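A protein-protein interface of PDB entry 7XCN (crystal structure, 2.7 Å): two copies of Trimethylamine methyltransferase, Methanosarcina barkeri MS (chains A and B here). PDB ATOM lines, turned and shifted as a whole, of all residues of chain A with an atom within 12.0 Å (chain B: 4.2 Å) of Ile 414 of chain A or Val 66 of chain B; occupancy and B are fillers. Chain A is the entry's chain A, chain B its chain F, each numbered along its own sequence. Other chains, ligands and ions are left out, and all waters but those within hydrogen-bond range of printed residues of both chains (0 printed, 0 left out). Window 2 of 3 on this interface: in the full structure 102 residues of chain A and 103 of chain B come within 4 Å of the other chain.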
ATOM      1  N   ALA A 405     -10.946 -19.950  42.572  1.00  0.00           N
ATOM      2  CA  ALA A 405     -10.933 -19.233  41.300  1.00  0.00           C
ATOM      3  C   ALA A 405     -11.979 -19.592  40.240  1.00  0.00           C
ATOM      4  O   ALA A 405     -11.667 -19.588  39.046  1.00  0.00           O
ATOM      5  CB  ALA A 405      -9.533 -19.354  40.696  1.00  0.00           C
ATOM      6  N   VAL A 406     -13.214 -19.868  40.649  1.00  0.00           N
ATOM      7  CA  VAL A 406     -14.233 -20.241  39.679  1.00  0.00           C
ATOM      8  C   VAL A 406     -14.314 -19.311  38.466  1.00  0.00           C
ATOM      9  O   VAL A 406     -14.387 -19.791  37.328  1.00  0.00           O
ATOM     10  CB  VAL A 406     -15.625 -20.347  40.336  1.00  0.00           C
ATOM     11  CG1 VAL A 406     -16.678 -20.742  39.292  1.00  0.00           C
ATOM     12  CG2 VAL A 406     -15.584 -21.380  41.446  1.00  0.00           C
ATOM     13  N   GLU A 407     -14.294 -17.996  38.693  1.00  0.00           N
ATOM     14  CA  GLU A 407     -14.365 -17.041  37.587  1.00  0.00           C
ATOM     15  C   GLU A 407     -13.234 -17.170  36.565  1.00  0.00           C
ATOM     16  O   GLU A 407     -13.435 -16.917  35.369  1.00  0.00           O
ATOM     17  CB  GLU A 407     -14.419 -15.614  38.119  1.00  0.00           C
ATOM     18  CG  GLU A 407     -15.765 -15.248  38.705  1.00  0.00           C
ATOM     19  CD  GLU A 407     -15.792 -13.857  39.302  1.00  0.00           C
ATOM     20  OE1 GLU A 407     -16.790 -13.529  39.982  1.00  0.00           O
ATOM     21  OE2 GLU A 407     -14.823 -13.095  39.092  1.00  0.00           O
ATOM     22  N   SER A 408     -12.048 -17.555  37.029  1.00  0.00           N
ATOM     23  CA  SER A 408     -10.913 -17.739  36.134  1.00  0.00           C
ATOM     24  C   SER A 408     -11.192 -18.941  35.249  1.00  0.00           C
ATOM     25  O   SER A 408     -10.940 -18.900  34.049  1.00  0.00           O
ATOM     26  CB  SER A 408      -9.639 -17.999  36.923  1.00  0.00           C
ATOM     27  OG  SER A 408      -9.417 -16.972  37.863  1.00  0.00           O
ATOM     28  N   ILE A 409     -11.701 -20.017  35.848  1.00  0.00           N
ATOM     29  CA  ILE A 409     -12.006 -21.220  35.092  1.00  0.00           C
ATOM     30  C   ILE A 409     -13.039 -20.820  34.042  1.00  0.00           C
ATOM     31  O   ILE A 409     -12.939 -21.190  32.875  1.00  0.00           O
ATOM     32  CB  ILE A 409     -12.612 -22.319  35.979  1.00  0.00           C
ATOM     33  CG1 ILE A 409     -11.731 -22.575  37.195  1.00  0.00           C
ATOM     34  CG2 ILE A 409     -12.754 -23.599  35.184  1.00  0.00           C
ATOM     35  CD1 ILE A 409     -10.396 -23.059  36.836  1.00  0.00           C
ATOM     36  N   GLN A 410     -14.029 -20.049  34.474  1.00  0.00           N
ATOM     37  CA  GLN A 410     -15.081 -19.583  33.586  1.00  0.00           C
ATOM     38  C   GLN A 410     -14.588 -18.563  32.555  1.00  0.00           C
ATOM     39  O   GLN A 410     -15.093 -18.531  31.432  1.00  0.00           O
ATOM     40  CB  GLN A 410     -16.240 -19.011  34.413  1.00  0.00           C
ATOM     41  CG  GLN A 410     -17.157 -20.097  34.900  1.00  0.00           C
ATOM     42  CD  GLN A 410     -18.017 -19.707  36.080  1.00  0.00           C
ATOM     43  OE1 GLN A 410     -18.862 -20.494  36.519  1.00  0.00           O
ATOM     44  NE2 GLN A 410     -17.809 -18.502  36.611  1.00  0.00           N
ATOM     45  N   LYS A 411     -13.609 -17.737  32.914  1.00  0.00           N
ATOM     46  CA  LYS A 411     -13.096 -16.762  31.958  1.00  0.00           C
ATOM     47  C   LYS A 411     -12.295 -17.452  30.857  1.00  0.00           C
ATOM     48  O   LYS A 411     -12.484 -17.171  29.672  1.00  0.00           O
ATOM     49  CB  LYS A 411     -12.209 -15.721  32.648  1.00  0.00           C
ATOM     50  CG  LYS A 411     -11.667 -14.658  31.693  1.00  0.00           C
ATOM     51  CD  LYS A 411     -10.741 -13.679  32.402  1.00  0.00           C
ATOM     52  CE  LYS A 411     -10.167 -12.644  31.439  1.00  0.00           C
ATOM     53  NZ  LYS A 411     -11.221 -11.755  30.867  1.00  0.00           N
ATOM     54  N   VAL A 412     -11.403 -18.354  31.258  1.00  0.00           N
ATOM     55  CA  VAL A 412     -10.557 -19.097  30.327  1.00  0.00           C
ATOM     56  C   VAL A 412     -11.350 -20.086  29.479  1.00  0.00           C
ATOM     57  O   VAL A 412     -10.986 -20.371  28.342  1.00  0.00           O
ATOM     58  CB  VAL A 412      -9.463 -19.865  31.092  1.00  0.00           C
ATOM     59  CG1 VAL A 412      -8.740 -20.810  30.164  1.00  0.00           C
ATOM     60  CG2 VAL A 412      -8.490 -18.885  31.716  1.00  0.00           C
ATOM     61  N   GLY A 413     -12.431 -20.614  30.046  1.00  0.00           N
ATOM     62  CA  GLY A 413     -13.267 -21.570  29.344  1.00  0.00           C
ATOM     63  C   GLY A 413     -12.607 -22.874  28.926  1.00  0.00           C
ATOM     64  O   GLY A 413     -11.453 -23.154  29.246  1.00  0.00           O
ATOM     65  N   ILE A 414     -13.365 -23.672  28.187  1.00  0.00           N
ATOM     66  CA  ILE A 414     -12.900 -24.961  27.691  1.00  0.00           C
ATOM     67  C   ILE A 414     -11.815 -24.843  26.619  1.00  0.00           C
ATOM     68  O   ILE A 414     -11.885 -23.985  25.736  1.00  0.00           O
ATOM     69  CB  ILE A 414     -14.071 -25.751  27.079  1.00  0.00           C
ATOM     70  CG1 ILE A 414     -15.160 -25.959  28.128  1.00  0.00           C
ATOM     71  CG2 ILE A 414     -13.577 -27.073  26.538  1.00  0.00           C
ATOM     72  CD1 ILE A 414     -16.466 -26.459  27.560  1.00  0.00           C
ATOM     73  N   GLY A 415     -10.817 -25.719  26.709  1.00  0.00           N
ATOM     74  CA  GLY A 415      -9.740 -25.755  25.734  1.00  0.00           C
ATOM     75  C   GLY A 415      -8.770 -24.594  25.619  1.00  0.00           C
ATOM     76  O   GLY A 415      -8.100 -24.468  24.603  1.00  0.00           O
ATOM     77  N   ASN A 416      -8.681 -23.738  26.630  1.00  0.00           N
ATOM     78  CA  ASN A 416      -7.746 -22.617  26.572  1.00  0.00           C
ATOM     79  C   ASN A 416      -6.725 -22.802  27.666  1.00  0.00           C
ATOM     80  O   ASN A 416      -6.670 -23.859  28.293  1.00  0.00           O
ATOM     81  CB  ASN A 416      -8.469 -21.288  26.765  1.00  0.00           C
ATOM     82  CG  ASN A 416      -9.407 -20.962  25.617  1.00  0.00           C
ATOM     83  OD1 ASN A 416     -10.020 -19.898  25.594  1.00  0.00           O
ATOM     84  ND2 ASN A 416      -9.522 -21.877  24.660  1.00  0.00           N
ATOM     85  N   ASN A 417      -5.898 -21.790  27.893  1.00  0.00           N
ATOM     86  CA  ASN A 417      -4.900 -21.901  28.946  1.00  0.00           C
ATOM     87  C   ASN A 417      -4.963 -20.658  29.799  1.00  0.00           C
ATOM     88  O   ASN A 417      -5.602 -19.686  29.422  1.00  0.00           O
ATOM     89  CB  ASN A 417      -3.489 -22.108  28.364  1.00  0.00           C
ATOM     90  CG  ASN A 417      -3.069 -21.004  27.420  1.00  0.00           C
ATOM     91  OD1 ASN A 417      -2.984 -19.835  27.802  1.00  0.00           O
ATOM     92  ND2 ASN A 417      -2.797 -21.373  26.175  1.00  0.00           N
ATOM     93  N   PHE A 418      -4.308 -20.696  30.955  1.00  0.00           N
ATOM     94  CA  PHE A 418      -4.325 -19.573  31.886  1.00  0.00           C
ATOM     95  C   PHE A 418      -3.088 -18.691  31.831  1.00  0.00           C
ATOM     96  O   PHE A 418      -2.953 -17.768  32.624  1.00  0.00           O
ATOM     97  CB  PHE A 418      -4.502 -20.095  33.312  1.00  0.00           C
ATOM     98  CG  PHE A 418      -5.841 -20.716  33.567  1.00  0.00           C
ATOM     99  CD1 PHE A 418      -6.261 -21.819  32.837  1.00  0.00           C
ATOM    100  CD2 PHE A 418      -6.691 -20.184  34.528  1.00  0.00           C
ATOM    101  CE1 PHE A 418      -7.506 -22.382  33.054  1.00  0.00           C
ATOM    102  CE2 PHE A 418      -7.942 -20.744  34.754  1.00  0.00           C
ATOM    103  CZ  PHE A 418      -8.350 -21.844  34.014  1.00  0.00           C
ATOM    104  N   LEU A 421      -3.377 -14.866  31.639  1.00  0.00           N
ATOM    105  CA  LEU A 421      -4.134 -14.263  32.732  1.00  0.00           C
ATOM    106  C   LEU A 421      -3.365 -13.304  33.626  1.00  0.00           C
ATOM    107  O   LEU A 421      -2.163 -13.466  33.853  1.00  0.00           O
ATOM    108  CB  LEU A 421      -4.758 -15.337  33.609  1.00  0.00           C
ATOM    109  CG  LEU A 421      -6.118 -15.838  33.148  1.00  0.00           C
ATOM    110  CD1 LEU A 421      -6.795 -16.565  34.307  1.00  0.00           C
ATOM    111  CD2 LEU A 421      -6.963 -14.659  32.684  1.00  0.00           C
ATOM    112  N   PRO B  40     -18.256 -23.533  32.626  1.00  0.00           N
ATOM    113  CA  PRO B  40     -18.613 -23.648  31.211  1.00  0.00           C
ATOM    114  C   PRO B  40     -19.102 -25.031  30.806  1.00  0.00           C
ATOM    115  O   PRO B  40     -19.483 -25.252  29.662  1.00  0.00           O
ATOM    116  CB  PRO B  40     -17.311 -23.306  30.519  1.00  0.00           C
ATOM    117  CG  PRO B  40     -16.328 -23.997  31.395  1.00  0.00           C
ATOM    118  CD  PRO B  40     -16.793 -23.593  32.786  1.00  0.00           C
ATOM    119  N   GLY B  41     -19.086 -25.968  31.743  1.00  0.00           N
ATOM    120  CA  GLY B  41     -19.521 -27.310  31.419  1.00  0.00           C
ATOM    121  C   GLY B  41     -18.354 -28.108  30.879  1.00  0.00           C
ATOM    122  O   GLY B  41     -17.199 -27.699  31.007  1.00  0.00           O
ATOM    123  N   ILE B  42     -18.645 -29.245  30.264  1.00  0.00           N
ATOM    124  CA  ILE B  42     -17.594 -30.089  29.733  1.00  0.00           C
ATOM    125  C   ILE B  42     -17.818 -30.484  28.282  1.00  0.00           C
ATOM    126  O   ILE B  42     -18.907 -30.915  27.902  1.00  0.00           O
ATOM    127  CB  ILE B  42     -17.442 -31.353  30.600  1.00  0.00           C
ATOM    128  CG1 ILE B  42     -16.778 -30.964  31.915  1.00  0.00           C
ATOM    129  CG2 ILE B  42     -16.620 -32.407  29.868  1.00  0.00           C
ATOM    130  CD1 ILE B  42     -16.553 -32.096  32.834  1.00  0.00           C
ATOM    131  N   GLN B  43     -16.769 -30.340  27.479  1.00  0.00           N
ATOM    132  CA  GLN B  43     -16.830 -30.679  26.064  1.00  0.00           C
ATOM    133  C   GLN B  43     -16.581 -32.167  25.831  1.00  0.00           C
ATOM    134  O   GLN B  43     -15.473 -32.660  26.025  1.00  0.00           O
ATOM    135  CB  GLN B  43     -15.807 -29.850  25.298  1.00  0.00           C
ATOM    136  CG  GLN B  43     -15.795 -30.109  23.805  1.00  0.00           C
ATOM    137  CD  GLN B  43     -15.007 -29.052  23.060  1.00  0.00           C
ATOM    138  OE1 GLN B  43     -15.376 -27.881  23.063  1.00  0.00           O
ATOM    139  NE2 GLN B  43     -13.914 -29.458  22.426  1.00  0.00           N
ATOM    140  N   GLU B  59     -27.753 -31.383  29.834  1.00  0.00           N
ATOM    141  CA  GLU B  59     -28.049 -30.477  28.738  1.00  0.00           C
ATOM    142  C   GLU B  59     -26.887 -30.638  27.766  1.00  0.00           C
ATOM    143  O   GLU B  59     -25.727 -30.471  28.146  1.00  0.00           O
ATOM    144  CB  GLU B  59     -28.093 -29.033  29.221  1.00  0.00           C
ATOM    145  CG  GLU B  59     -29.142 -28.744  30.265  1.00  0.00           C
ATOM    146  CD  GLU B  59     -29.085 -27.306  30.740  1.00  0.00           C
ATOM    147  OE1 GLU B  59     -29.263 -26.397  29.898  1.00  0.00           O
ATOM    148  OE2 GLU B  59     -28.856 -27.086  31.952  1.00  0.00           O
ATOM    149  N   VAL B  60     -27.190 -30.969  26.516  1.00  0.00           N
ATOM    150  CA  VAL B  60     -26.140 -31.154  25.523  1.00  0.00           C
ATOM    151  C   VAL B  60     -26.333 -30.283  24.294  1.00  0.00           C
ATOM    152  O   VAL B  60     -27.314 -30.415  23.573  1.00  0.00           O
ATOM    153  CB  VAL B  60     -26.057 -32.616  25.061  1.00  0.00           C
ATOM    154  CG1 VAL B  60     -24.865 -32.796  24.151  1.00  0.00           C
ATOM    155  CG2 VAL B  60     -25.960 -33.530  26.257  1.00  0.00           C
ATOM    156  N   ASN B  61     -25.378 -29.392  24.073  1.00  0.00           N
ATOM    157  CA  ASN B  61     -25.376 -28.486  22.937  1.00  0.00           C
ATOM    158  C   ASN B  61     -24.648 -29.212  21.798  1.00  0.00           C
ATOM    159  O   ASN B  61     -23.430 -29.365  21.838  1.00  0.00           O
ATOM    160  CB  ASN B  61     -24.621 -27.216  23.326  1.00  0.00           C
ATOM    161  CG  ASN B  61     -24.462 -26.256  22.180  1.00  0.00           C
ATOM    162  OD1 ASN B  61     -24.125 -26.651  21.066  1.00  0.00           O
ATOM    163  ND2 ASN B  61     -24.685 -24.980  22.450  1.00  0.00           N
ATOM    164  N   THR B  64     -21.657 -27.080  19.934  1.00  0.00           N
ATOM    165  CA  THR B  64     -20.413 -26.883  20.661  1.00  0.00           C
ATOM    166  C   THR B  64     -19.910 -28.177  21.285  1.00  0.00           C
ATOM    167  O   THR B  64     -18.741 -28.283  21.664  1.00  0.00           O
ATOM    168  CB  THR B  64     -20.604 -25.852  21.779  1.00  0.00           C
ATOM    169  OG1 THR B  64     -21.457 -26.399  22.790  1.00  0.00           O
ATOM    170  CG2 THR B  64     -21.252 -24.592  21.231  1.00  0.00           C
ATOM    171  N   ASN B  65     -20.804 -29.158  21.377  1.00  0.00           N
ATOM    172  CA  ASN B  65     -20.511 -30.460  21.977  1.00  0.00           C
ATOM    173  C   ASN B  65     -20.274 -30.373  23.485  1.00  0.00           C
ATOM    174  O   ASN B  65     -19.733 -31.305  24.090  1.00  0.00           O
ATOM    175  CB  ASN B  65     -19.302 -31.112  21.320  1.00  0.00           C
ATOM    176  CG  ASN B  65     -19.644 -31.763  20.004  1.00  0.00           C
ATOM    177  OD1 ASN B  65     -20.801 -32.104  19.757  1.00  0.00           O
ATOM    178  ND2 ASN B  65     -18.636 -31.961  19.156  1.00  0.00           N
ATOM    179  N   VAL B  66     -20.685 -29.256  24.086  1.00  0.00           N
ATOM    180  CA  VAL B  66     -20.527 -29.063  25.513  1.00  0.00           C
ATOM    181  C   VAL B  66     -21.670 -29.704  26.284  1.00  0.00           C
ATOM    182  O   VAL B  66     -22.838 -29.581  25.909  1.00  0.00           O
ATOM    183  CB  VAL B  66     -20.459 -27.575  25.869  1.00  0.00           C
ATOM    184  CG1 VAL B  66     -20.473 -27.396  27.378  1.00  0.00           C
ATOM    185  CG2 VAL B  66     -19.211 -26.976  25.279  1.00  0.00           C
ATOM    186  N   VAL B  67     -21.312 -30.393  27.361  1.00  0.00           N
ATOM    187  CA  VAL B  67     -22.271 -31.073  28.217  1.00  0.00           C
ATOM    188  C   VAL B  67     -22.294 -30.418  29.594  1.00  0.00           C
ATOM    189  O   VAL B  67     -21.245 -30.126  30.163  1.00  0.00           O
ATOM    190  CB  VAL B  67     -21.891 -32.558  28.369  1.00  0.00           C
ATOM    191  CG1 VAL B  67     -22.746 -33.221  29.436  1.00  0.00           C
ATOM    192  CG2 VAL B  67     -22.055 -33.253  27.035  1.00  0.00           C
ATOM    193  N   PRO B 223      -7.995 -27.909  29.701  1.00  0.00           N
ATOM    194  CA  PRO B 223      -9.104 -27.849  30.656  1.00  0.00           C
ATOM    195  C   PRO B 223     -10.517 -28.230  30.188  1.00  0.00           C
ATOM    196  O   PRO B 223     -10.967 -27.855  29.102  1.00  0.00           O
ATOM    197  CB  PRO B 223      -9.056 -26.400  31.120  1.00  0.00           C
ATOM    198  CG  PRO B 223      -8.724 -25.691  29.862  1.00  0.00           C
ATOM    199  CD  PRO B 223      -7.630 -26.555  29.249  1.00  0.00           C
ATOM    200  N   LEU B 224     -11.194 -28.989  31.040  1.00  0.00           N
ATOM    201  CA  LEU B 224     -12.585 -29.389  30.851  1.00  0.00           C
ATOM    202  C   LEU B 224     -13.102 -30.021  29.562  1.00  0.00           C
ATOM    203  O   LEU B 224     -14.049 -29.513  28.959  1.00  0.00           O
ATOM    204  CB  LEU B 224     -13.462 -28.186  31.174  1.00  0.00           C
ATOM    205  CG  LEU B 224     -13.112 -27.506  32.495  1.00  0.00           C
ATOM    206  CD1 LEU B 224     -13.704 -26.110  32.525  1.00  0.00           C
ATOM    207  CD2 LEU B 224     -13.609 -28.353  33.654  1.00  0.00           C
ATOM    208  N   GLU B 225     -12.522 -31.134  29.137  1.00  0.00           N
ATOM    209  CA  GLU B 225     -13.038 -31.784  27.949  1.00  0.00           C
ATOM    210  C   GLU B 225     -12.572 -33.227  27.803  1.00  0.00           C
ATOM    211  O   GLU B 225     -11.425 -33.554  28.065  1.00  0.00           O
ATOM    212  CB  GLU B 225     -12.698 -30.959  26.702  1.00  0.00           C
ATOM    213  CG  GLU B 225     -11.319 -31.174  26.094  1.00  0.00           C
ATOM    214  CD  GLU B 225     -11.121 -30.353  24.820  1.00  0.00           C
ATOM    215  OE1 GLU B 225     -10.927 -29.120  24.930  1.00  0.00           O
ATOM    216  OE2 GLU B 225     -11.176 -30.940  23.713  1.00  0.00           O
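The backbone carbonyl oxygen (O) of Pro 223 of chain B lies within hydrogen-bond range of the backbone NH (N) of Gly 415 of chain A (3.2 Å).
No position is printed for both chains. Of the 12 pairs that touch across the chains among the printed residues, none has its exchanged pair printed and touching as well.
Ile 414 of chain A touches just these residues of chain B: Pro 40 (3.9 Å), Gly 41 (3.7 Å), Gln 43 (3.8 Å), Val 66 (3.6 Å), Pro 223 (3.7 Å), Leu 224 (3.5 Å) and Glu 225 (3.7 Å). Val 66 of chain B touches just one residue of chain A: Ile 414 (3.6 Å). Pro 40 of chain B touches just one residue of chain A: Ile 414. Gly 41 of chain B touches just one residue of chain A: Ile 414. No residue of chain A comes within 4 Å of Ile 42 of chain B. No residue of chain A comes within 4 Å of Val 60 of chain B. No residue of chain A comes within 4 Å of Asn 61 of chain B. No residue of chain A comes within 4 Å of Thr 64 of chain B. No residue of chain A comes within 4 Å of Asn 65 of chain B. No residue of chain A comes within 4 Å of Val 67 of chain B. Of the printed residues of chain A, Pro 223 of chain B touches Gly 413 (3.8 Å), Ile 414 (3.7 Å), Gly 415 (3.2 Å) and Asn 416 (3.0 Å). Printed residues of chain A within 4 Å of Leu 224 of chain B: Ile 409 and Ile 414. Printed residues of chain B within 4 Å of Gly 413 of chain A: Pro 223. Printed residues of chain B within 4 Å of Asn 416 of chain A: Pro 223 (3.0 Å). Printed residues of chain B within 4 Å of Gly 415 of chain A: Pro 223 (3.2 Å) and Glu 225 (3.7 Å). Of the printed residues of chain B, Ile 409 of chain A touches Leu 224. The nearest printed residue of chain B that does not touch Asn 416 of chain A is Glu 225 of chain B (6.1 Å).
Ile 409 of chain A touches Leu 224 of chain B. Gly 413 of chain A touches Pro 223 of chain B (O to CG, 3.8 Å). CD1 of Ile 414 of chain A touches O of Pro 40 of chain B, at 3.9 Å. O of Gly 41 of chain B touches CD1 of Ile 414 of chain A, 3.7 Å away. Ile 414 of chain A touches Gln 43 of chain B (CG2 to CB, 3.8 Å). Ile 414 of chain A touches Pro 223 of chain B (CG2 to O, 3.7 Å). O of Leu 224 of chain B touches CG2 of Ile 414 of chain A, 3.5 Å away. Ile 414 of chain A touches Glu 225 of chain B (CG2 to OE1, 3.7 Å). OE1 of Glu 225 of chain B touches CA of Gly 415 of chain A (3.7 Å). CD of Pro 223 of chain B touches O of Asn 416 of chain A (3.0 Å).
The side-chain amide oxygen of Asn 416 of chain A lies close to the backbone carbonyl oxygen of Val 412 of chain A. O of Ile 414 of chain A lies within hydrogen-bond range of ND2 of Asn 416 of chain A, at 3.3 Å. The backbone NH of Gln 43 of chain B lies within hydrogen-bond range of the backbone carbonyl oxygen of Leu 224 of chain B. The side-chain carboxylate (OE2) of Glu 225 of chain B sits at hydrogen-bond distance from the side-chain amide nitrogen (NE2) of Gln 43 of chain B, at 3.4 Å. N of Asn 61 of chain B sits at hydrogen-bond distance from O of Val 66 of chain B, 3.1 Å away. OG1 of Thr 64 of chain B lies close to N of Val 66 of chain B (3.2 Å).
Hydrophobic or aromatic side chains of chain B that line the printed part of chain A: Pro 40, Val 66, Pro 223 and Leu 224. Of the 15 printed residues of chain A, 5 touch a printed residue of chain B. Hydrophobic or aromatic side chains of chain A that line the printed part of chain B: Ile 409 and Ile 414. Among the printed residues, 12 pairs touch across the chains. Among the printed residues, no Asp or Glu carboxylate lies within 4 Å of a Lys or Arg side-chain nitrogen of the other chain.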
